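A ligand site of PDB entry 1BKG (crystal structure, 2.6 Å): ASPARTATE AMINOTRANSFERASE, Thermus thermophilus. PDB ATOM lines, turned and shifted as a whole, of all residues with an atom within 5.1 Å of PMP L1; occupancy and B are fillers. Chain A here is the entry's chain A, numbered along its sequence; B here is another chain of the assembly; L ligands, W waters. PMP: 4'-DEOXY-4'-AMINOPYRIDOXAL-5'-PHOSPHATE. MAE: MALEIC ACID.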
ATOM      1  N   GLY A  39      18.303 -20.320 -16.107  1.00  0.00           N
ATOM      2  CA  GLY A  39      19.254 -19.397 -16.694  1.00  0.00           C
ATOM      3  C   GLY A  39      20.577 -20.112 -16.811  1.00  0.00           C
ATOM      4  O   GLY A  39      21.653 -19.529 -16.667  1.00  0.00           O
ATOM      5  N   VAL A  98      34.485 -15.704  -7.761  1.00  0.00           N
ATOM      6  CA  VAL A  98      33.495 -16.758  -7.543  1.00  0.00           C
ATOM      7  C   VAL A  98      32.279 -16.466  -8.424  1.00  0.00           C
ATOM      8  O   VAL A  98      31.231 -16.032  -7.939  1.00  0.00           O
ATOM      9  CB  VAL A  98      33.086 -16.849  -6.047  1.00  0.00           C
ATOM     10  CG1 VAL A  98      32.039 -17.907  -5.878  1.00  0.00           C
ATOM     11  CG2 VAL A  98      34.283 -17.148  -5.178  1.00  0.00           C
ATOM     12  N   GLY A  99      32.417 -16.701  -9.731  1.00  0.00           N
ATOM     13  CA  GLY A  99      31.346 -16.417 -10.673  1.00  0.00           C
ATOM     14  C   GLY A  99      31.423 -14.958 -11.141  1.00  0.00           C
ATOM     15  O   GLY A  99      32.145 -14.135 -10.553  1.00  0.00           O
ATOM     16  N   GLY A 100      30.761 -14.643 -12.248  1.00  0.00           N
ATOM     17  CA  GLY A 100      30.744 -13.280 -12.746  1.00  0.00           C
ATOM     18  C   GLY A 100      30.000 -12.374 -11.771  1.00  0.00           C
ATOM     19  O   GLY A 100      30.225 -11.170 -11.740  1.00  0.00           O
ATOM     20  N   LYS A 101      29.114 -12.947 -10.976  1.00  0.00           N
ATOM     21  CA  LYS A 101      28.361 -12.181  -9.994  1.00  0.00           C
ATOM     22  C   LYS A 101      29.291 -11.567  -8.947  1.00  0.00           C
ATOM     23  O   LYS A 101      29.076 -10.451  -8.540  1.00  0.00           O
ATOM     24  CB  LYS A 101      27.304 -13.046  -9.306  1.00  0.00           C
ATOM     25  CG  LYS A 101      26.424 -12.298  -8.338  1.00  0.00           C
ATOM     26  CD  LYS A 101      25.319 -13.163  -7.796  1.00  0.00           C
ATOM     27  CE  LYS A 101      24.229 -13.370  -8.823  1.00  0.00           C
ATOM     28  NZ  LYS A 101      23.098 -14.182  -8.282  1.00  0.00           N
ATOM     29  N   LEU A 104      31.136  -8.514 -10.309  1.00  0.00           N
ATOM     30  CA  LEU A 104      30.288  -7.324 -10.259  1.00  0.00           C
ATOM     31  C   LEU A 104      30.099  -6.819  -8.817  1.00  0.00           C
ATOM     32  O   LEU A 104      30.156  -5.606  -8.553  1.00  0.00           O
ATOM     33  CB  LEU A 104      28.920  -7.628 -10.852  1.00  0.00           C
ATOM     34  CG  LEU A 104      28.829  -7.891 -12.348  1.00  0.00           C
ATOM     35  CD1 LEU A 104      27.570  -8.661 -12.710  1.00  0.00           C
ATOM     36  CD2 LEU A 104      28.877  -6.589 -13.085  1.00  0.00           C
ATOM     37  N   TRP A 125      19.067  -6.988 -15.608  1.00  0.00           N
ATOM     38  CA  TRP A 125      19.127  -8.213 -14.846  1.00  0.00           C
ATOM     39  C   TRP A 125      18.863  -7.903 -13.367  1.00  0.00           C
ATOM     40  O   TRP A 125      19.418  -6.986 -12.776  1.00  0.00           O
ATOM     41  CB  TRP A 125      20.502  -8.885 -15.052  1.00  0.00           C
ATOM     42  CG  TRP A 125      20.771 -10.121 -14.255  1.00  0.00           C
ATOM     43  CD1 TRP A 125      19.947 -11.179 -14.084  1.00  0.00           C
ATOM     44  CD2 TRP A 125      21.946 -10.407 -13.509  1.00  0.00           C
ATOM     45  NE1 TRP A 125      20.530 -12.120 -13.274  1.00  0.00           N
ATOM     46  CE2 TRP A 125      21.772 -11.670 -12.911  1.00  0.00           C
ATOM     47  CE3 TRP A 125      23.142  -9.729 -13.276  1.00  0.00           C
ATOM     48  CZ2 TRP A 125      22.742 -12.256 -12.105  1.00  0.00           C
ATOM     49  CZ3 TRP A 125      24.109 -10.316 -12.495  1.00  0.00           C
ATOM     50  CH2 TRP A 125      23.896 -11.563 -11.914  1.00  0.00           C
ATOM     51  N   TYR A 128      21.590  -6.233 -10.777  1.00  0.00           N
ATOM     52  CA  TYR A 128      22.290  -4.938 -10.900  1.00  0.00           C
ATOM     53  C   TYR A 128      21.826  -3.908  -9.882  1.00  0.00           C
ATOM     54  O   TYR A 128      22.639  -3.370  -9.153  1.00  0.00           O
ATOM     55  CB  TYR A 128      22.167  -4.340 -12.308  1.00  0.00           C
ATOM     56  CG  TYR A 128      22.856  -5.100 -13.422  1.00  0.00           C
ATOM     57  CD1 TYR A 128      24.060  -5.778 -13.204  1.00  0.00           C
ATOM     58  CD2 TYR A 128      22.281  -5.148 -14.700  1.00  0.00           C
ATOM     59  CE1 TYR A 128      24.672  -6.505 -14.236  1.00  0.00           C
ATOM     60  CE2 TYR A 128      22.888  -5.862 -15.736  1.00  0.00           C
ATOM     61  CZ  TYR A 128      24.082  -6.538 -15.496  1.00  0.00           C
ATOM     62  OH  TYR A 128      24.663  -7.240 -16.509  1.00  0.00           O
ATOM     63  N   ASN A 171      25.061  -4.596 -20.886  1.00  0.00           N
ATOM     64  CA  ASN A 171      24.993  -6.058 -20.907  1.00  0.00           C
ATOM     65  C   ASN A 171      24.592  -6.565 -22.298  1.00  0.00           C
ATOM     66  O   ASN A 171      23.423  -6.499 -22.673  1.00  0.00           O
ATOM     67  CB  ASN A 171      23.994  -6.521 -19.832  1.00  0.00           C
ATOM     68  CG  ASN A 171      23.735  -8.002 -19.833  1.00  0.00           C
ATOM     69  OD1 ASN A 171      22.614  -8.420 -19.613  1.00  0.00           O
ATOM     70  ND2 ASN A 171      24.777  -8.807 -20.058  1.00  0.00           N
ATOM     71  N   ASN A 175      20.423 -10.065 -20.918  1.00  0.00           N
ATOM     72  CA  ASN A 175      19.532 -10.875 -20.087  1.00  0.00           C
ATOM     73  C   ASN A 175      18.702  -9.723 -19.467  1.00  0.00           C
ATOM     74  O   ASN A 175      19.275  -8.894 -18.752  1.00  0.00           O
ATOM     75  CB  ASN A 175      20.319 -11.606 -19.002  1.00  0.00           C
ATOM     76  CG  ASN A 175      19.419 -12.337 -18.007  1.00  0.00           C
ATOM     77  OD1 ASN A 175      18.201 -12.246 -18.076  1.00  0.00           O
ATOM     78  ND2 ASN A 175      20.024 -13.036 -17.073  1.00  0.00           N
ATOM     79  N   ASP A 203      29.149  -6.268 -19.063  1.00  0.00           N
ATOM     80  CA  ASP A 203      28.858  -7.650 -18.667  1.00  0.00           C
ATOM     81  C   ASP A 203      28.676  -8.509 -19.932  1.00  0.00           C
ATOM     82  O   ASP A 203      27.600  -8.525 -20.549  1.00  0.00           O
ATOM     83  CB  ASP A 203      27.590  -7.652 -17.809  1.00  0.00           C
ATOM     84  CG  ASP A 203      27.319  -8.979 -17.122  1.00  0.00           C
ATOM     85  OD1 ASP A 203      28.087  -9.944 -17.265  1.00  0.00           O
ATOM     86  OD2 ASP A 203      26.290  -9.048 -16.428  1.00  0.00           O
ATOM     87  N   ILE A 205      29.148 -12.138 -20.188  1.00  0.00           N
ATOM     88  CA  ILE A 205      29.029 -13.606 -19.991  1.00  0.00           C
ATOM     89  C   ILE A 205      28.336 -14.367 -21.124  1.00  0.00           C
ATOM     90  O   ILE A 205      28.623 -15.554 -21.338  1.00  0.00           O
ATOM     91  CB  ILE A 205      28.339 -14.067 -18.652  1.00  0.00           C
ATOM     92  CG1 ILE A 205      27.545 -12.942 -18.043  1.00  0.00           C
ATOM     93  CG2 ILE A 205      29.302 -14.684 -17.645  1.00  0.00           C
ATOM     94  CD1 ILE A 205      26.389 -12.543 -18.866  1.00  0.00           C
ATOM     95  N   TYR A 206      27.414 -13.743 -21.860  1.00  0.00           N
ATOM     96  CA  TYR A 206      26.759 -14.455 -22.953  1.00  0.00           C
ATOM     97  C   TYR A 206      27.425 -14.252 -24.315  1.00  0.00           C
ATOM     98  O   TYR A 206      26.810 -14.533 -25.334  1.00  0.00           O
ATOM     99  CB  TYR A 206      25.292 -14.053 -23.061  1.00  0.00           C
ATOM    100  CG  TYR A 206      24.469 -14.387 -21.838  1.00  0.00           C
ATOM    101  CD1 TYR A 206      24.083 -15.698 -21.579  1.00  0.00           C
ATOM    102  CD2 TYR A 206      24.153 -13.408 -20.911  1.00  0.00           C
ATOM    103  CE1 TYR A 206      23.409 -16.009 -20.419  1.00  0.00           C
ATOM    104  CE2 TYR A 206      23.479 -13.728 -19.754  1.00  0.00           C
ATOM    105  CZ  TYR A 206      23.112 -15.030 -19.519  1.00  0.00           C
ATOM    106  OH  TYR A 206      22.473 -15.340 -18.359  1.00  0.00           O
ATOM    107  N   ALA A 233      30.637 -19.775 -16.826  1.00  0.00           N
ATOM    108  CA  ALA A 233      29.269 -20.234 -16.643  1.00  0.00           C
ATOM    109  C   ALA A 233      28.426 -20.581 -17.865  1.00  0.00           C
ATOM    110  O   ALA A 233      27.940 -21.711 -17.987  1.00  0.00           O
ATOM    111  CB  ALA A 233      28.533 -19.265 -15.781  1.00  0.00           C
ATOM    112  N   LYS A 234      28.203 -19.633 -18.774  1.00  0.00           N
ATOM    113  CA  LYS A 234      27.352 -19.901 -19.924  1.00  0.00           C
ATOM    114  C   LYS A 234      28.052 -20.590 -21.086  1.00  0.00           C
ATOM    115  O   LYS A 234      27.506 -21.504 -21.682  1.00  0.00           O
ATOM    116  CB  LYS A 234      26.698 -18.618 -20.415  1.00  0.00           C
ATOM    117  CG  LYS A 234      26.156 -17.776 -19.290  1.00  0.00           C
ATOM    118  CD  LYS A 234      25.160 -18.520 -18.409  1.00  0.00           C
ATOM    119  CE  LYS A 234      24.960 -17.714 -17.149  1.00  0.00           C
ATOM    120  NZ  LYS A 234      23.891 -18.263 -16.248  1.00  0.00           N
ATOM    121  N   THR A 239      28.099 -23.542 -14.631  1.00  0.00           N
ATOM    122  CA  THR A 239      27.390 -22.696 -13.665  1.00  0.00           C
ATOM    123  C   THR A 239      27.657 -23.050 -12.224  1.00  0.00           C
ATOM    124  O   THR A 239      27.914 -22.164 -11.409  1.00  0.00           O
ATOM    125  CB  THR A 239      25.894 -22.673 -13.902  1.00  0.00           C
ATOM    126  OG1 THR A 239      25.437 -23.998 -14.128  1.00  0.00           O
ATOM    127  CG2 THR A 239      25.564 -21.840 -15.110  1.00  0.00           C
ATOM    128  N   ARG A 242      31.307 -22.042 -10.226  1.00  0.00           N
ATOM    129  CA  ARG A 242      31.511 -20.708  -9.677  1.00  0.00           C
ATOM    130  C   ARG A 242      32.827 -20.062 -10.053  1.00  0.00           C
ATOM    131  O   ARG A 242      33.653 -19.789  -9.181  1.00  0.00           O
ATOM    132  CB  ARG A 242      31.351 -20.735  -8.149  1.00  0.00           C
ATOM    133  CG  ARG A 242      30.091 -21.447  -7.619  1.00  0.00           C
ATOM    134  CD  ARG A 242      28.831 -21.041  -8.375  1.00  0.00           C
ATOM    135  NE  ARG A 242      28.568 -19.620  -8.277  1.00  0.00           N
ATOM    136  CZ  ARG A 242      28.284 -18.813  -9.296  1.00  0.00           C
ATOM    137  NH1 ARG A 242      28.233 -19.297 -10.537  1.00  0.00           N
ATOM    138  NH2 ARG A 242      28.098 -17.506  -9.088  1.00  0.00           N
ATOM    139  N   ILE A 243      33.051 -19.865 -11.346  1.00  0.00           N
ATOM    140  CA  ILE A 243      34.286 -19.216 -11.790  1.00  0.00           C
ATOM    141  C   ILE A 243      33.996 -18.108 -12.760  1.00  0.00           C
ATOM    142  O   ILE A 243      33.446 -18.336 -13.808  1.00  0.00           O
ATOM    143  CB  ILE A 243      35.284 -20.190 -12.459  1.00  0.00           C
ATOM    144  CG1 ILE A 243      35.947 -21.087 -11.419  1.00  0.00           C
ATOM    145  CG2 ILE A 243      36.355 -19.417 -13.216  1.00  0.00           C
ATOM    146  CD1 ILE A 243      36.975 -20.388 -10.545  1.00  0.00           C
ATOM    147  N   TYR A 322      17.231 -16.262 -23.685  1.00  0.00           N
ATOM    148  CA  TYR A 322      15.993 -15.737 -23.102  1.00  0.00           C
ATOM    149  C   TYR A 322      15.169 -15.004 -24.132  1.00  0.00           C
ATOM    150  O   TYR A 322      15.689 -14.521 -25.128  1.00  0.00           O
ATOM    151  CB  TYR A 322      16.290 -14.754 -21.969  1.00  0.00           C
ATOM    152  CG  TYR A 322      17.336 -15.215 -20.981  1.00  0.00           C
ATOM    153  CD1 TYR A 322      17.044 -16.161 -19.998  1.00  0.00           C
ATOM    154  CD2 TYR A 322      18.629 -14.706 -21.038  1.00  0.00           C
ATOM    155  CE1 TYR A 322      18.014 -16.599 -19.101  1.00  0.00           C
ATOM    156  CE2 TYR A 322      19.598 -15.135 -20.137  1.00  0.00           C
ATOM    157  CZ  TYR A 322      19.287 -16.078 -19.164  1.00  0.00           C
ATOM    158  OH  TYR A 322      20.228 -16.524 -18.275  1.00  0.00           O
ATOM    159  N   TYR B  64      23.911 -24.804 -10.753  1.00  0.00           N
ATOM    160  CA  TYR B  64      23.852 -23.912  -9.581  1.00  0.00           C
ATOM    161  C   TYR B  64      23.194 -24.587  -8.383  1.00  0.00           C
ATOM    162  O   TYR B  64      22.208 -25.290  -8.547  1.00  0.00           O
ATOM    163  CB  TYR B  64      23.004 -22.684  -9.869  1.00  0.00           C
ATOM    164  CG  TYR B  64      23.511 -21.668 -10.833  1.00  0.00           C
ATOM    165  CD1 TYR B  64      24.719 -21.011 -10.629  1.00  0.00           C
ATOM    166  CD2 TYR B  64      22.749 -21.297 -11.922  1.00  0.00           C
ATOM    167  CE1 TYR B  64      25.140 -19.998 -11.502  1.00  0.00           C
ATOM    168  CE2 TYR B  64      23.152 -20.320 -12.782  1.00  0.00           C
ATOM    169  CZ  TYR B  64      24.343 -19.677 -12.571  1.00  0.00           C
ATOM    170  OH  TYR B  64      24.709 -18.763 -13.491  1.00  0.00           O
ATOM    171  N   THR B 265      26.112 -16.318  -5.496  1.00  0.00           N
ATOM    172  CA  THR B 265      25.012 -17.242  -5.785  1.00  0.00           C
ATOM    173  C   THR B 265      25.040 -18.363  -4.754  1.00  0.00           C
ATOM    174  O   THR B 265      24.207 -18.402  -3.845  1.00  0.00           O
ATOM    175  CB  THR B 265      25.017 -17.796  -7.211  1.00  0.00           C
ATOM    176  OG1 THR B 265      24.833 -16.723  -8.143  1.00  0.00           O
ATOM    177  CG2 THR B 265      23.861 -18.768  -7.398  1.00  0.00           C
HETATM  178  N1  PMP L   1      25.604 -11.260 -15.775  1.00  0.00           N
HETATM  179  C2  PMP L   1      24.420 -11.713 -16.274  1.00  0.00           C
HETATM  180  C2A PMP L   1      23.592 -10.816 -17.230  1.00  0.00           C
HETATM  181  C3  PMP L   1      23.963 -12.956 -15.912  1.00  0.00           C
HETATM  182  O3  PMP L   1      22.777 -13.414 -16.398  1.00  0.00           O
HETATM  183  C4  PMP L   1      24.730 -13.742 -15.027  1.00  0.00           C
HETATM  184  C4A PMP L   1      24.220 -15.103 -14.603  1.00  0.00           C
HETATM  185  N4A PMP L   1      23.628 -15.692 -15.684  1.00  0.00           N
HETATM  186  C5  PMP L   1      25.957 -13.249 -14.520  1.00  0.00           C
HETATM  187  C6  PMP L   1      26.361 -12.017 -14.911  1.00  0.00           C
HETATM  188  C5A PMP L   1      26.870 -14.042 -13.526  1.00  0.00           C
HETATM  189  O4P PMP L   1      26.868 -15.449 -13.667  1.00  0.00           O
HETATM  190  P   PMP L   1      27.715 -16.365 -12.746  1.00  0.00           P
HETATM  191  O1P PMP L   1      28.969 -16.376 -13.481  1.00  0.00           O
HETATM  192  O2P PMP L   1      26.934 -17.712 -12.802  1.00  0.00           O
HETATM  193  O3P PMP L   1      27.781 -15.964 -11.364  1.00  0.00           O
HETATM  194  C1  MAE L   2      21.073 -15.587 -11.730  1.00  0.00           C
HETATM  195  O1  MAE L   2      20.138 -14.763 -11.670  1.00  0.00           O
HETATM  196  O2  MAE L   2      21.819 -15.809 -10.757  1.00  0.00           O
HETATM  197  C2  MAE L   2      21.351 -16.346 -13.058  1.00  0.00           C
HETATM  198  C3  MAE L   2      20.581 -16.389 -14.148  1.00  0.00           C
HETATM  199  C4  MAE L   2      19.249 -15.683 -14.326  1.00  0.00           C
HETATM  200  O3  MAE L   2      19.221 -14.505 -14.726  1.00  0.00           O
HETATM  201  O4  MAE L   2      18.212 -16.304 -14.073  1.00  0.00           O
HETATM  202  O   HOH W   1      30.900 -17.751 -14.668  1.00  0.00           O
HETATM  203  O   HOH W   2      24.853 -16.427 -10.820  1.00  0.00           O
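NE1 of Trp 125 lies within hydrogen-bond range of O3 of MAE L2 (3.1 Å).
The side-chain hydroxyl (OH) of Tyr 206 lies within hydrogen-bond range of an oxygen (O3) of PMP L1 (2.8 Å).
OD2 of Asp 203 is in hydrogen-bond range of N1 of PMP L1, 2.4 Å away.
O3 of PMP L1 is in hydrogen-bond range of ND2 of Asn 175, at 2.9 Å.
An oxygen (O2P) of PMP L1 sits at hydrogen-bond distance from the side-chain hydroxyl (OH) of Tyr 64 of chain B (2.6 Å).
An oxygen (O2) of MAE L2 lies within salt-bridge range of the side-chain amino group of Lys 101, 3.2 Å away.
N of Lys 101 is in hydrogen-bond range of O3P of PMP L1, at 3.3 Å.
O1P of PMP L1 is in hydrogen-bond range of N of Gly 100 (2.8 Å).
An oxygen (O3P) of PMP L1 lies within salt-bridge range of the guanidinium group of Arg 242, at 2.8 Å.
The side-chain amino group of Lys 234 sits close to a nitrogen (N4A) of PMP L1, 2.6 Å away.
The side-chain amide nitrogen (ND2) of Asn 175 is in hydrogen-bond range of an oxygen (O3) of MAE L2.
The backbone carbonyl oxygen (O) of Gly 39 sits at hydrogen-bond distance from the side-chain amino group (NZ) of Lys 234.
NZ of Lys 101 is in hydrogen-bond range of OG1 of Thr 265 of chain B, at 3.1 Å.
The side-chain hydroxyl of Tyr 128 sits at hydrogen-bond distance from the side-chain carboxylate of Asp 203, 2.4 Å away.
OH of Tyr 64 of chain B lies within hydrogen-bond range of NZ of Lys 234 (2.9 Å).
OG1 of Thr 265 of chain B is in hydrogen-bond range of NH2 of Arg 242 (3.5 Å).
The backbone NH (N) of Gly 99 lies within hydrogen-bond range of the backbone carbonyl oxygen (O) of Arg 242.
ND2 of Asn 171 sits at hydrogen-bond distance from O of Asp 203 (2.9 Å).
The side-chain hydroxyl (OH) of Tyr 206 lies within hydrogen-bond range of the side-chain hydroxyl (OH) of Tyr 322 (2.5 Å).
CA of Gly 99 touches O3P of PMP L1, at 3.7 Å.
CZ3 of Trp 125 touches C6 of PMP L1 (3.7 Å).
Tyr 128 touches PMP L1.
Asn 171 touches PMP L1.
CD1 of Ile 205 touches C2 of PMP L1, at 3.4 Å.
Ala 233 touches PMP L1 (CB to O1P, 3.7 Å).
Hydrophobic or aromatic side chains that line PMP L1: Trp 125, Ile 205, Tyr 206, Ala 233 and Tyr 64 of chain B.
Of the 21 residues printed, 14 come within 4 Å of PMP L1.
Water W1 lies within hydrogen-bond range of O1P of PMP L1 (2.7 Å), O of Ile 243 (2.8 Å) and N of Ala 233 (3.0 Å).
Water W2 lies within hydrogen-bond range of the side-chain hydroxyl of Thr 265 of chain B (2.7 Å), an oxygen (O3P) of PMP L1 (3.0 Å) and an oxygen (O2) of MAE L2 (3.1 Å).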
